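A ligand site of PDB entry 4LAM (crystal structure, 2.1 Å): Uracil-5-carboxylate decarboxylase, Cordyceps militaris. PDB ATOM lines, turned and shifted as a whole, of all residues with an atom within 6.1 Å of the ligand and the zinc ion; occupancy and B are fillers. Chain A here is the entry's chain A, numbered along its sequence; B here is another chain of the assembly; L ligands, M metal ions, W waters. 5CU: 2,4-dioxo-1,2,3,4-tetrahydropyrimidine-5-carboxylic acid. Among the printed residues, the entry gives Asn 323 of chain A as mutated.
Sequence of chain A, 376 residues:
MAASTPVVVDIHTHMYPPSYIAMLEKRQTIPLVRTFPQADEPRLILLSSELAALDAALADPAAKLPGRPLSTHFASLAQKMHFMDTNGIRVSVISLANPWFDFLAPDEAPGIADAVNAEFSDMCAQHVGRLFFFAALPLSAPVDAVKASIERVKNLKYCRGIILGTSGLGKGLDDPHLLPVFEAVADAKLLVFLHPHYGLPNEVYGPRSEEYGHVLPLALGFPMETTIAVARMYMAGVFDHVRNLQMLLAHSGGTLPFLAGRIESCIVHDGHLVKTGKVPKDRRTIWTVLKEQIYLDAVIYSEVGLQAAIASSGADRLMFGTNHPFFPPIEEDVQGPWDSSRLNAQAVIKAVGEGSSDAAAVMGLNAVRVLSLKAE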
ATOM      1  N   HIS A  12     -17.093  14.743  -9.511  1.00  0.00           N
ATOM      2  CA  HIS A  12     -16.786  15.631 -10.621  1.00  0.00           C
ATOM      3  C   HIS A  12     -16.708  17.029 -10.042  1.00  0.00           C
ATOM      4  O   HIS A  12     -17.696  17.772 -10.057  1.00  0.00           O
ATOM      5  CB  HIS A  12     -17.860  15.531 -11.710  1.00  0.00           C
ATOM      6  CG  HIS A  12     -17.506  16.244 -12.979  1.00  0.00           C
ATOM      7  ND1 HIS A  12     -17.946  15.800 -14.218  1.00  0.00           N
ATOM      8  CD2 HIS A  12     -16.767  17.349 -13.221  1.00  0.00           C
ATOM      9  CE1 HIS A  12     -17.494  16.620 -15.158  1.00  0.00           C
ATOM     10  NE2 HIS A  12     -16.774  17.566 -14.584  1.00  0.00           N
ATOM     11  N   HIS A  14     -13.729  20.293  -9.235  1.00  0.00           N
ATOM     12  CA  HIS A  14     -12.407  20.700  -9.681  1.00  0.00           C
ATOM     13  C   HIS A  14     -11.763  21.765  -8.814  1.00  0.00           C
ATOM     14  O   HIS A  14     -12.444  22.481  -8.066  1.00  0.00           O
ATOM     15  CB  HIS A  14     -12.474  21.260 -11.110  1.00  0.00           C
ATOM     16  CG  HIS A  14     -13.049  20.311 -12.121  1.00  0.00           C
ATOM     17  ND1 HIS A  14     -12.525  19.053 -12.339  1.00  0.00           N
ATOM     18  CD2 HIS A  14     -14.080  20.453 -12.983  1.00  0.00           C
ATOM     19  CE1 HIS A  14     -13.219  18.456 -13.299  1.00  0.00           C
ATOM     20  NE2 HIS A  14     -14.167  19.284 -13.701  1.00  0.00           N
ATOM     21  N   TYR A  16      -8.085  24.575  -9.266  1.00  0.00           N
ATOM     22  CA  TYR A  16      -6.762  24.946  -9.745  1.00  0.00           C
ATOM     23  C   TYR A  16      -6.039  25.469  -8.520  1.00  0.00           C
ATOM     24  O   TYR A  16      -6.402  26.523  -8.009  1.00  0.00           O
ATOM     25  CB  TYR A  16      -6.819  26.073 -10.777  1.00  0.00           C
ATOM     26  CG  TYR A  16      -7.529  25.770 -12.083  1.00  0.00           C
ATOM     27  CD1 TYR A  16      -7.019  24.837 -12.973  1.00  0.00           C
ATOM     28  CD2 TYR A  16      -8.689  26.442 -12.438  1.00  0.00           C
ATOM     29  CE1 TYR A  16      -7.658  24.569 -14.175  1.00  0.00           C
ATOM     30  CE2 TYR A  16      -9.336  26.183 -13.632  1.00  0.00           C
ATOM     31  CZ  TYR A  16      -8.806  25.246 -14.500  1.00  0.00           C
ATOM     32  OH  TYR A  16      -9.447  24.977 -15.687  1.00  0.00           O
ATOM     33  N   LEU A  46      -9.182  29.314 -21.339  1.00  0.00           N
ATOM     34  CA  LEU A  46      -8.677  27.939 -21.416  1.00  0.00           C
ATOM     35  C   LEU A  46      -8.789  27.315 -22.788  1.00  0.00           C
ATOM     36  O   LEU A  46      -8.027  26.414 -23.134  1.00  0.00           O
ATOM     37  CB  LEU A  46      -9.449  27.049 -20.444  1.00  0.00           C
ATOM     38  CG  LEU A  46      -9.453  27.434 -18.961  1.00  0.00           C
ATOM     39  CD1 LEU A  46     -10.431  26.551 -18.223  1.00  0.00           C
ATOM     40  CD2 LEU A  46      -8.055  27.318 -18.375  1.00  0.00           C
ATOM     41  N   LEU A  47      -9.750  27.788 -23.576  1.00  0.00           N
ATOM     42  CA  LEU A  47     -10.238  27.032 -24.721  1.00  0.00           C
ATOM     43  C   LEU A  47      -9.822  27.591 -26.067  1.00  0.00           C
ATOM     44  O   LEU A  47      -9.701  28.807 -26.248  1.00  0.00           O
ATOM     45  CB  LEU A  47     -11.761  26.937 -24.686  1.00  0.00           C
ATOM     46  CG  LEU A  47     -12.444  26.497 -23.387  1.00  0.00           C
ATOM     47  CD1 LEU A  47     -13.942  26.423 -23.620  1.00  0.00           C
ATOM     48  CD2 LEU A  47     -11.896  25.171 -22.889  1.00  0.00           C
ATOM     49  N   ARG A  68     -13.966  33.301 -19.231  1.00  0.00           N
ATOM     50  CA  ARG A  68     -14.988  33.372 -18.184  1.00  0.00           C
ATOM     51  C   ARG A  68     -14.390  33.988 -16.931  1.00  0.00           C
ATOM     52  O   ARG A  68     -13.157  34.015 -16.787  1.00  0.00           O
ATOM     53  CB  ARG A  68     -15.507  31.967 -17.884  1.00  0.00           C
ATOM     54  CG  ARG A  68     -16.356  31.388 -19.014  1.00  0.00           C
ATOM     55  CD  ARG A  68     -16.546  29.887 -18.873  1.00  0.00           C
ATOM     56  NE  ARG A  68     -15.313  29.147 -19.141  1.00  0.00           N
ATOM     57  CZ  ARG A  68     -15.219  27.820 -19.130  1.00  0.00           C
ATOM     58  NH1 ARG A  68     -16.300  27.074 -18.886  1.00  0.00           N
ATOM     59  NH2 ARG A  68     -14.057  27.223 -19.381  1.00  0.00           N
ATOM     60  N   ALA A  97      -8.519  20.749 -12.954  1.00  0.00           N
ATOM     61  CA  ALA A  97      -9.386  20.949 -14.102  1.00  0.00           C
ATOM     62  C   ALA A  97      -8.574  21.038 -15.393  1.00  0.00           C
ATOM     63  O   ALA A  97      -7.350  21.100 -15.368  1.00  0.00           O
ATOM     64  CB  ALA A  97     -10.241  22.197 -13.924  1.00  0.00           C
ATOM     65  N   ASN A  98      -9.284  21.037 -16.521  1.00  0.00           N
ATOM     66  CA  ASN A  98      -8.656  21.127 -17.830  1.00  0.00           C
ATOM     67  C   ASN A  98      -7.879  22.421 -17.982  1.00  0.00           C
ATOM     68  O   ASN A  98      -8.275  23.442 -17.435  1.00  0.00           O
ATOM     69  CB  ASN A  98      -9.721  21.029 -18.938  1.00  0.00           C
ATOM     70  CG  ASN A  98     -10.888  21.984 -18.717  1.00  0.00           C
ATOM     71  OD1 ASN A  98     -11.517  21.974 -17.656  1.00  0.00           O
ATOM     72  ND2 ASN A  98     -11.171  22.832 -19.697  1.00  0.00           N
ATOM     73  N   PHE A 193     -10.510   8.880 -14.942  1.00  0.00           N
ATOM     74  CA  PHE A 193     -11.585   9.837 -15.191  1.00  0.00           C
ATOM     75  C   PHE A 193     -11.297  10.570 -16.507  1.00  0.00           C
ATOM     76  O   PHE A 193     -10.383  11.403 -16.571  1.00  0.00           O
ATOM     77  CB  PHE A 193     -11.650  10.816 -14.009  1.00  0.00           C
ATOM     78  CG  PHE A 193     -12.788  11.815 -14.080  1.00  0.00           C
ATOM     79  CD1 PHE A 193     -13.892  11.622 -14.896  1.00  0.00           C
ATOM     80  CD2 PHE A 193     -12.744  12.967 -13.290  1.00  0.00           C
ATOM     81  CE1 PHE A 193     -14.923  12.552 -14.937  1.00  0.00           C
ATOM     82  CE2 PHE A 193     -13.769  13.895 -13.323  1.00  0.00           C
ATOM     83  CZ  PHE A 193     -14.859  13.692 -14.139  1.00  0.00           C
ATOM     84  N   HIS A 195     -12.118  13.310 -19.240  1.00  0.00           N
ATOM     85  CA  HIS A 195     -12.795  14.606 -19.189  1.00  0.00           C
ATOM     86  C   HIS A 195     -12.473  15.410 -20.444  1.00  0.00           C
ATOM     87  O   HIS A 195     -11.349  15.378 -20.940  1.00  0.00           O
ATOM     88  CB  HIS A 195     -12.315  15.380 -17.943  1.00  0.00           C
ATOM     89  CG  HIS A 195     -13.128  16.598 -17.621  1.00  0.00           C
ATOM     90  ND1 HIS A 195     -13.081  17.746 -18.369  1.00  0.00           N
ATOM     91  CD2 HIS A 195     -13.981  16.855 -16.593  1.00  0.00           C
ATOM     92  CE1 HIS A 195     -13.886  18.658 -17.853  1.00  0.00           C
ATOM     93  NE2 HIS A 195     -14.440  18.138 -16.766  1.00  0.00           N
ATOM     94  N   PRO A 196     -13.464  16.126 -20.985  1.00  0.00           N
ATOM     95  CA  PRO A 196     -13.217  16.909 -22.207  1.00  0.00           C
ATOM     96  C   PRO A 196     -12.423  18.208 -21.991  1.00  0.00           C
ATOM     97  O   PRO A 196     -12.127  18.580 -20.853  1.00  0.00           O
ATOM     98  CB  PRO A 196     -14.627  17.226 -22.699  1.00  0.00           C
ATOM     99  CG  PRO A 196     -15.479  17.224 -21.451  1.00  0.00           C
ATOM    100  CD  PRO A 196     -14.893  16.106 -20.610  1.00  0.00           C
ATOM    101  N   HIS A 197     -12.087  18.862 -23.098  1.00  0.00           N
ATOM    102  CA  HIS A 197     -11.374  20.149 -23.093  1.00  0.00           C
ATOM    103  C   HIS A 197     -11.132  20.692 -24.493  1.00  0.00           C
ATOM    104  O   HIS A 197     -11.334  21.881 -24.738  1.00  0.00           O
ATOM    105  CB  HIS A 197      -9.996  20.036 -22.436  1.00  0.00           C
ATOM    106  CG  HIS A 197      -9.152  21.256 -22.669  1.00  0.00           C
ATOM    107  ND1 HIS A 197      -9.377  22.447 -22.014  1.00  0.00           N
ATOM    108  CD2 HIS A 197      -8.143  21.497 -23.537  1.00  0.00           C
ATOM    109  CE1 HIS A 197      -8.519  23.357 -22.440  1.00  0.00           C
ATOM    110  NE2 HIS A 197      -7.757  22.799 -23.361  1.00  0.00           N
ATOM    111  N   LEU A 218     -19.274  24.246 -25.006  1.00  0.00           N
ATOM    112  CA  LEU A 218     -19.478  23.592 -23.708  1.00  0.00           C
ATOM    113  C   LEU A 218     -20.600  22.560 -23.751  1.00  0.00           C
ATOM    114  O   LEU A 218     -20.469  21.470 -23.209  1.00  0.00           O
ATOM    115  CB  LEU A 218     -19.733  24.618 -22.596  1.00  0.00           C
ATOM    116  CG  LEU A 218     -18.586  25.591 -22.321  1.00  0.00           C
ATOM    117  CD1 LEU A 218     -18.906  26.488 -21.124  1.00  0.00           C
ATOM    118  CD2 LEU A 218     -17.285  24.827 -22.085  1.00  0.00           C
ATOM    119  N   PHE A 222     -17.732  19.658 -25.846  1.00  0.00           N
ATOM    120  CA  PHE A 222     -17.210  18.815 -24.751  1.00  0.00           C
ATOM    121  C   PHE A 222     -17.739  17.369 -24.764  1.00  0.00           C
ATOM    122  O   PHE A 222     -16.953  16.435 -24.848  1.00  0.00           O
ATOM    123  CB  PHE A 222     -17.467  19.467 -23.383  1.00  0.00           C
ATOM    124  CG  PHE A 222     -16.386  20.422 -22.937  1.00  0.00           C
ATOM    125  CD1 PHE A 222     -15.549  21.041 -23.864  1.00  0.00           C
ATOM    126  CD2 PHE A 222     -16.206  20.704 -21.599  1.00  0.00           C
ATOM    127  CE1 PHE A 222     -14.561  21.924 -23.457  1.00  0.00           C
ATOM    128  CE2 PHE A 222     -15.213  21.584 -21.171  1.00  0.00           C
ATOM    129  CZ  PHE A 222     -14.390  22.194 -22.100  1.00  0.00           C
ATOM    130  N   ALA A 250     -16.875  11.596 -18.027  1.00  0.00           N
ATOM    131  CA  ALA A 250     -17.489  12.891 -17.742  1.00  0.00           C
ATOM    132  C   ALA A 250     -18.854  13.047 -18.427  1.00  0.00           C
ATOM    133  O   ALA A 250     -19.068  12.547 -19.537  1.00  0.00           O
ATOM    134  CB  ALA A 250     -16.566  14.013 -18.200  1.00  0.00           C
ATOM    135  N   HIS A 251     -19.762  13.755 -17.767  1.00  0.00           N
ATOM    136  CA  HIS A 251     -21.036  14.159 -18.372  1.00  0.00           C
ATOM    137  C   HIS A 251     -21.840  12.969 -18.890  1.00  0.00           C
ATOM    138  O   HIS A 251     -22.313  12.978 -20.029  1.00  0.00           O
ATOM    139  CB  HIS A 251     -20.786  15.180 -19.479  1.00  0.00           C
ATOM    140  CG  HIS A 251     -19.830  16.266 -19.066  1.00  0.00           C
ATOM    141  ND1 HIS A 251     -18.677  16.559 -19.757  1.00  0.00           N
ATOM    142  CD2 HIS A 251     -19.850  17.095 -17.998  1.00  0.00           C
ATOM    143  CE1 HIS A 251     -18.036  17.535 -19.151  1.00  0.00           C
ATOM    144  NE2 HIS A 251     -18.725  17.879 -18.076  1.00  0.00           N
ATOM    145  N   TYR A 301     -27.931  16.996 -16.288  1.00  0.00           N
ATOM    146  CA  TYR A 301     -28.885  18.109 -16.206  1.00  0.00           C
ATOM    147  C   TYR A 301     -30.321  17.805 -16.645  1.00  0.00           C
ATOM    148  O   TYR A 301     -31.073  18.723 -16.947  1.00  0.00           O
ATOM    149  CB  TYR A 301     -28.382  19.321 -16.995  1.00  0.00           C
ATOM    150  CG  TYR A 301     -26.969  19.745 -16.623  1.00  0.00           C
ATOM    151  CD1 TYR A 301     -26.739  20.548 -15.519  1.00  0.00           C
ATOM    152  CD2 TYR A 301     -25.879  19.335 -17.388  1.00  0.00           C
ATOM    153  CE1 TYR A 301     -25.447  20.930 -15.171  1.00  0.00           C
ATOM    154  CE2 TYR A 301     -24.593  19.718 -17.047  1.00  0.00           C
ATOM    155  CZ  TYR A 301     -24.390  20.523 -15.946  1.00  0.00           C
ATOM    156  OH  TYR A 301     -23.112  20.897 -15.614  1.00  0.00           O
ATOM    157  N   ASN A 323     -19.632  19.303 -10.966  1.00  0.00           N
ATOM    158  CA  ASN A 323     -18.757  20.157 -11.768  1.00  0.00           C
ATOM    159  C   ASN A 323     -18.496  21.527 -11.110  1.00  0.00           C
ATOM    160  O   ASN A 323     -18.264  22.529 -11.799  1.00  0.00           O
ATOM    161  CB  ASN A 323     -19.287  20.344 -13.185  1.00  0.00           C
ATOM    162  CG  ASN A 323     -18.259  20.955 -14.115  1.00  0.00           C
ATOM    163  OD1 ASN A 323     -17.081  20.594 -14.079  1.00  0.00           O
ATOM    164  ND2 ASN A 323     -18.699  21.894 -14.949  1.00  0.00           N
ATOM    165  N   PHE A 326     -17.457  25.381 -11.844  1.00  0.00           N
ATOM    166  CA  PHE A 326     -17.872  25.930 -13.129  1.00  0.00           C
ATOM    167  C   PHE A 326     -19.373  26.198 -13.106  1.00  0.00           C
ATOM    168  O   PHE A 326     -20.092  25.673 -12.250  1.00  0.00           O
ATOM    169  CB  PHE A 326     -17.497  24.972 -14.263  1.00  0.00           C
ATOM    170  CG  PHE A 326     -16.034  24.944 -14.583  1.00  0.00           C
ATOM    171  CD1 PHE A 326     -15.471  25.906 -15.410  1.00  0.00           C
ATOM    172  CD2 PHE A 326     -15.199  23.972 -14.044  1.00  0.00           C
ATOM    173  CE1 PHE A 326     -14.108  25.890 -15.709  1.00  0.00           C
ATOM    174  CE2 PHE A 326     -13.836  23.946 -14.345  1.00  0.00           C
ATOM    175  CZ  PHE A 326     -13.295  24.909 -15.166  1.00  0.00           C
ATOM    176  N   PHE A 327     -19.834  27.036 -14.018  1.00  0.00           N
ATOM    177  CA  PHE A 327     -21.256  27.386 -14.114  1.00  0.00           C
ATOM    178  C   PHE A 327     -21.850  27.898 -12.803  1.00  0.00           C
ATOM    179  O   PHE A 327     -22.829  27.329 -12.313  1.00  0.00           O
ATOM    180  CB  PHE A 327     -22.077  26.191 -14.592  1.00  0.00           C
ATOM    181  CG  PHE A 327     -21.629  25.615 -15.911  1.00  0.00           C
ATOM    182  CD1 PHE A 327     -21.867  26.305 -17.097  1.00  0.00           C
ATOM    183  CD2 PHE A 327     -20.983  24.392 -15.963  1.00  0.00           C
ATOM    184  CE1 PHE A 327     -21.467  25.780 -18.315  1.00  0.00           C
ATOM    185  CE2 PHE A 327     -20.569  23.855 -17.181  1.00  0.00           C
ATOM    186  CZ  PHE A 327     -20.815  24.545 -18.361  1.00  0.00           C
ATOM    187  N   ARG B 262     -28.273  19.607 -20.949  1.00  0.00           N
ATOM    188  CA  ARG B 262     -26.973  20.287 -20.901  1.00  0.00           C
ATOM    189  C   ARG B 262     -27.027  21.623 -21.665  1.00  0.00           C
ATOM    190  O   ARG B 262     -26.500  22.631 -21.195  1.00  0.00           O
ATOM    191  CB  ARG B 262     -25.864  19.388 -21.472  1.00  0.00           C
ATOM    192  CG  ARG B 262     -24.466  20.006 -21.357  1.00  0.00           C
ATOM    193  CD  ARG B 262     -23.351  19.114 -21.905  1.00  0.00           C
ATOM    194  NE  ARG B 262     -22.046  19.764 -21.695  1.00  0.00           N
ATOM    195  CZ  ARG B 262     -21.389  19.774 -20.536  1.00  0.00           C
ATOM    196  NH1 ARG B 262     -21.890  19.163 -19.469  1.00  0.00           N
ATOM    197  NH2 ARG B 262     -20.230  20.415 -20.441  1.00  0.00           N
HETATM  198  O53 5CU L   1     -18.600  21.173 -18.006  1.00  0.00           O
HETATM  199  C51 5CU L   1     -17.454  20.997 -17.494  1.00  0.00           C
HETATM  200  O52 5CU L   1     -17.227  19.917 -16.912  1.00  0.00           O
HETATM  201  C5  5CU L   1     -16.441  21.937 -17.729  1.00  0.00           C
HETATM  202  C4  5CU L   1     -15.158  21.871 -17.170  1.00  0.00           C
HETATM  203  O4  5CU L   1     -14.826  21.009 -16.352  1.00  0.00           O
HETATM  204  N3  5CU L   1     -14.204  22.838 -17.522  1.00  0.00           N
HETATM  205  C2  5CU L   1     -14.535  23.840 -18.423  1.00  0.00           C
HETATM  206  O2  5CU L   1     -13.710  24.699 -18.750  1.00  0.00           O
HETATM  207  N1  5CU L   1     -15.830  23.873 -18.952  1.00  0.00           N
HETATM  208  C6  5CU L   1     -16.721  22.967 -18.629  1.00  0.00           C
HETATM  209 ZN    ZN M   1     -15.730  19.400 -15.384  1.00  0.00          ZN
HETATM  210  O   HOH W   1     -20.880  19.795 -16.929  1.00  0.00           O
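Merely in contact with the ligand: Phe 222 (3.2 Å), Phe 326 (3.3 Å), Phe 327 (3.4 Å), Leu 218 (3.6 Å) and Leu 46 (3.8 Å). Within 4 Å of the ligand: His 12, His 14, Leu 46, Arg 68, Asn 98, His 195, Leu 218, Phe 222, His 251, Asn 323, Phe 326, Phe 327 and Arg 262 of chain B. The nearest printed residue that does not touch the ligand is Leu 47 (4.5 Å).
NH2 of Arg 262 of chain B is in salt-bridge range of O53 of the ligand. The side-chain amide oxygen (OD1) of Asn 98 lies within hydrogen-bond range of a nitrogen (N3) of the ligand, 2.8 Å away. NE2 of His 251 sits at hydrogen-bond distance from O53 of the ligand (3.3 Å). O2 of the ligand lies within hydrogen-bond range of NH2 of Arg 68.
Water W1 lies within hydrogen-bond range of NH1 of Arg 262 of chain B (2.8 Å), OH of Tyr 301 (2.8 Å), O53 of the ligand (2.9 Å) and NE2 of His 251 (3.1 Å).
NE of Arg 262 of chain B is in hydrogen-bond range of O of Leu 218, 2.8 Å away. A ring nitrogen (ND1) of His 197 is in hydrogen-bond range of the side-chain amide nitrogen (ND2) of Asn 98 (3.0 Å). OH of Tyr 16 lies within hydrogen-bond range of O of Asn 98, 2.6 Å away.
O4 of the ligand is bound to the zinc ion (2.1 Å). O52 of the ligand is bound to the zinc ion (2.2 Å). The zinc ion is bound by the side-chain amide oxygen (OD1) of Asn 323, at 2.2 Å. The zinc ion is bound by NE2 of His 12 (2.3 Å). NE2 of His 195 binds the zinc ion, 2.3 Å away. A ring nitrogen (NE2) of His 14 binds the zinc ion (2.3 Å).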
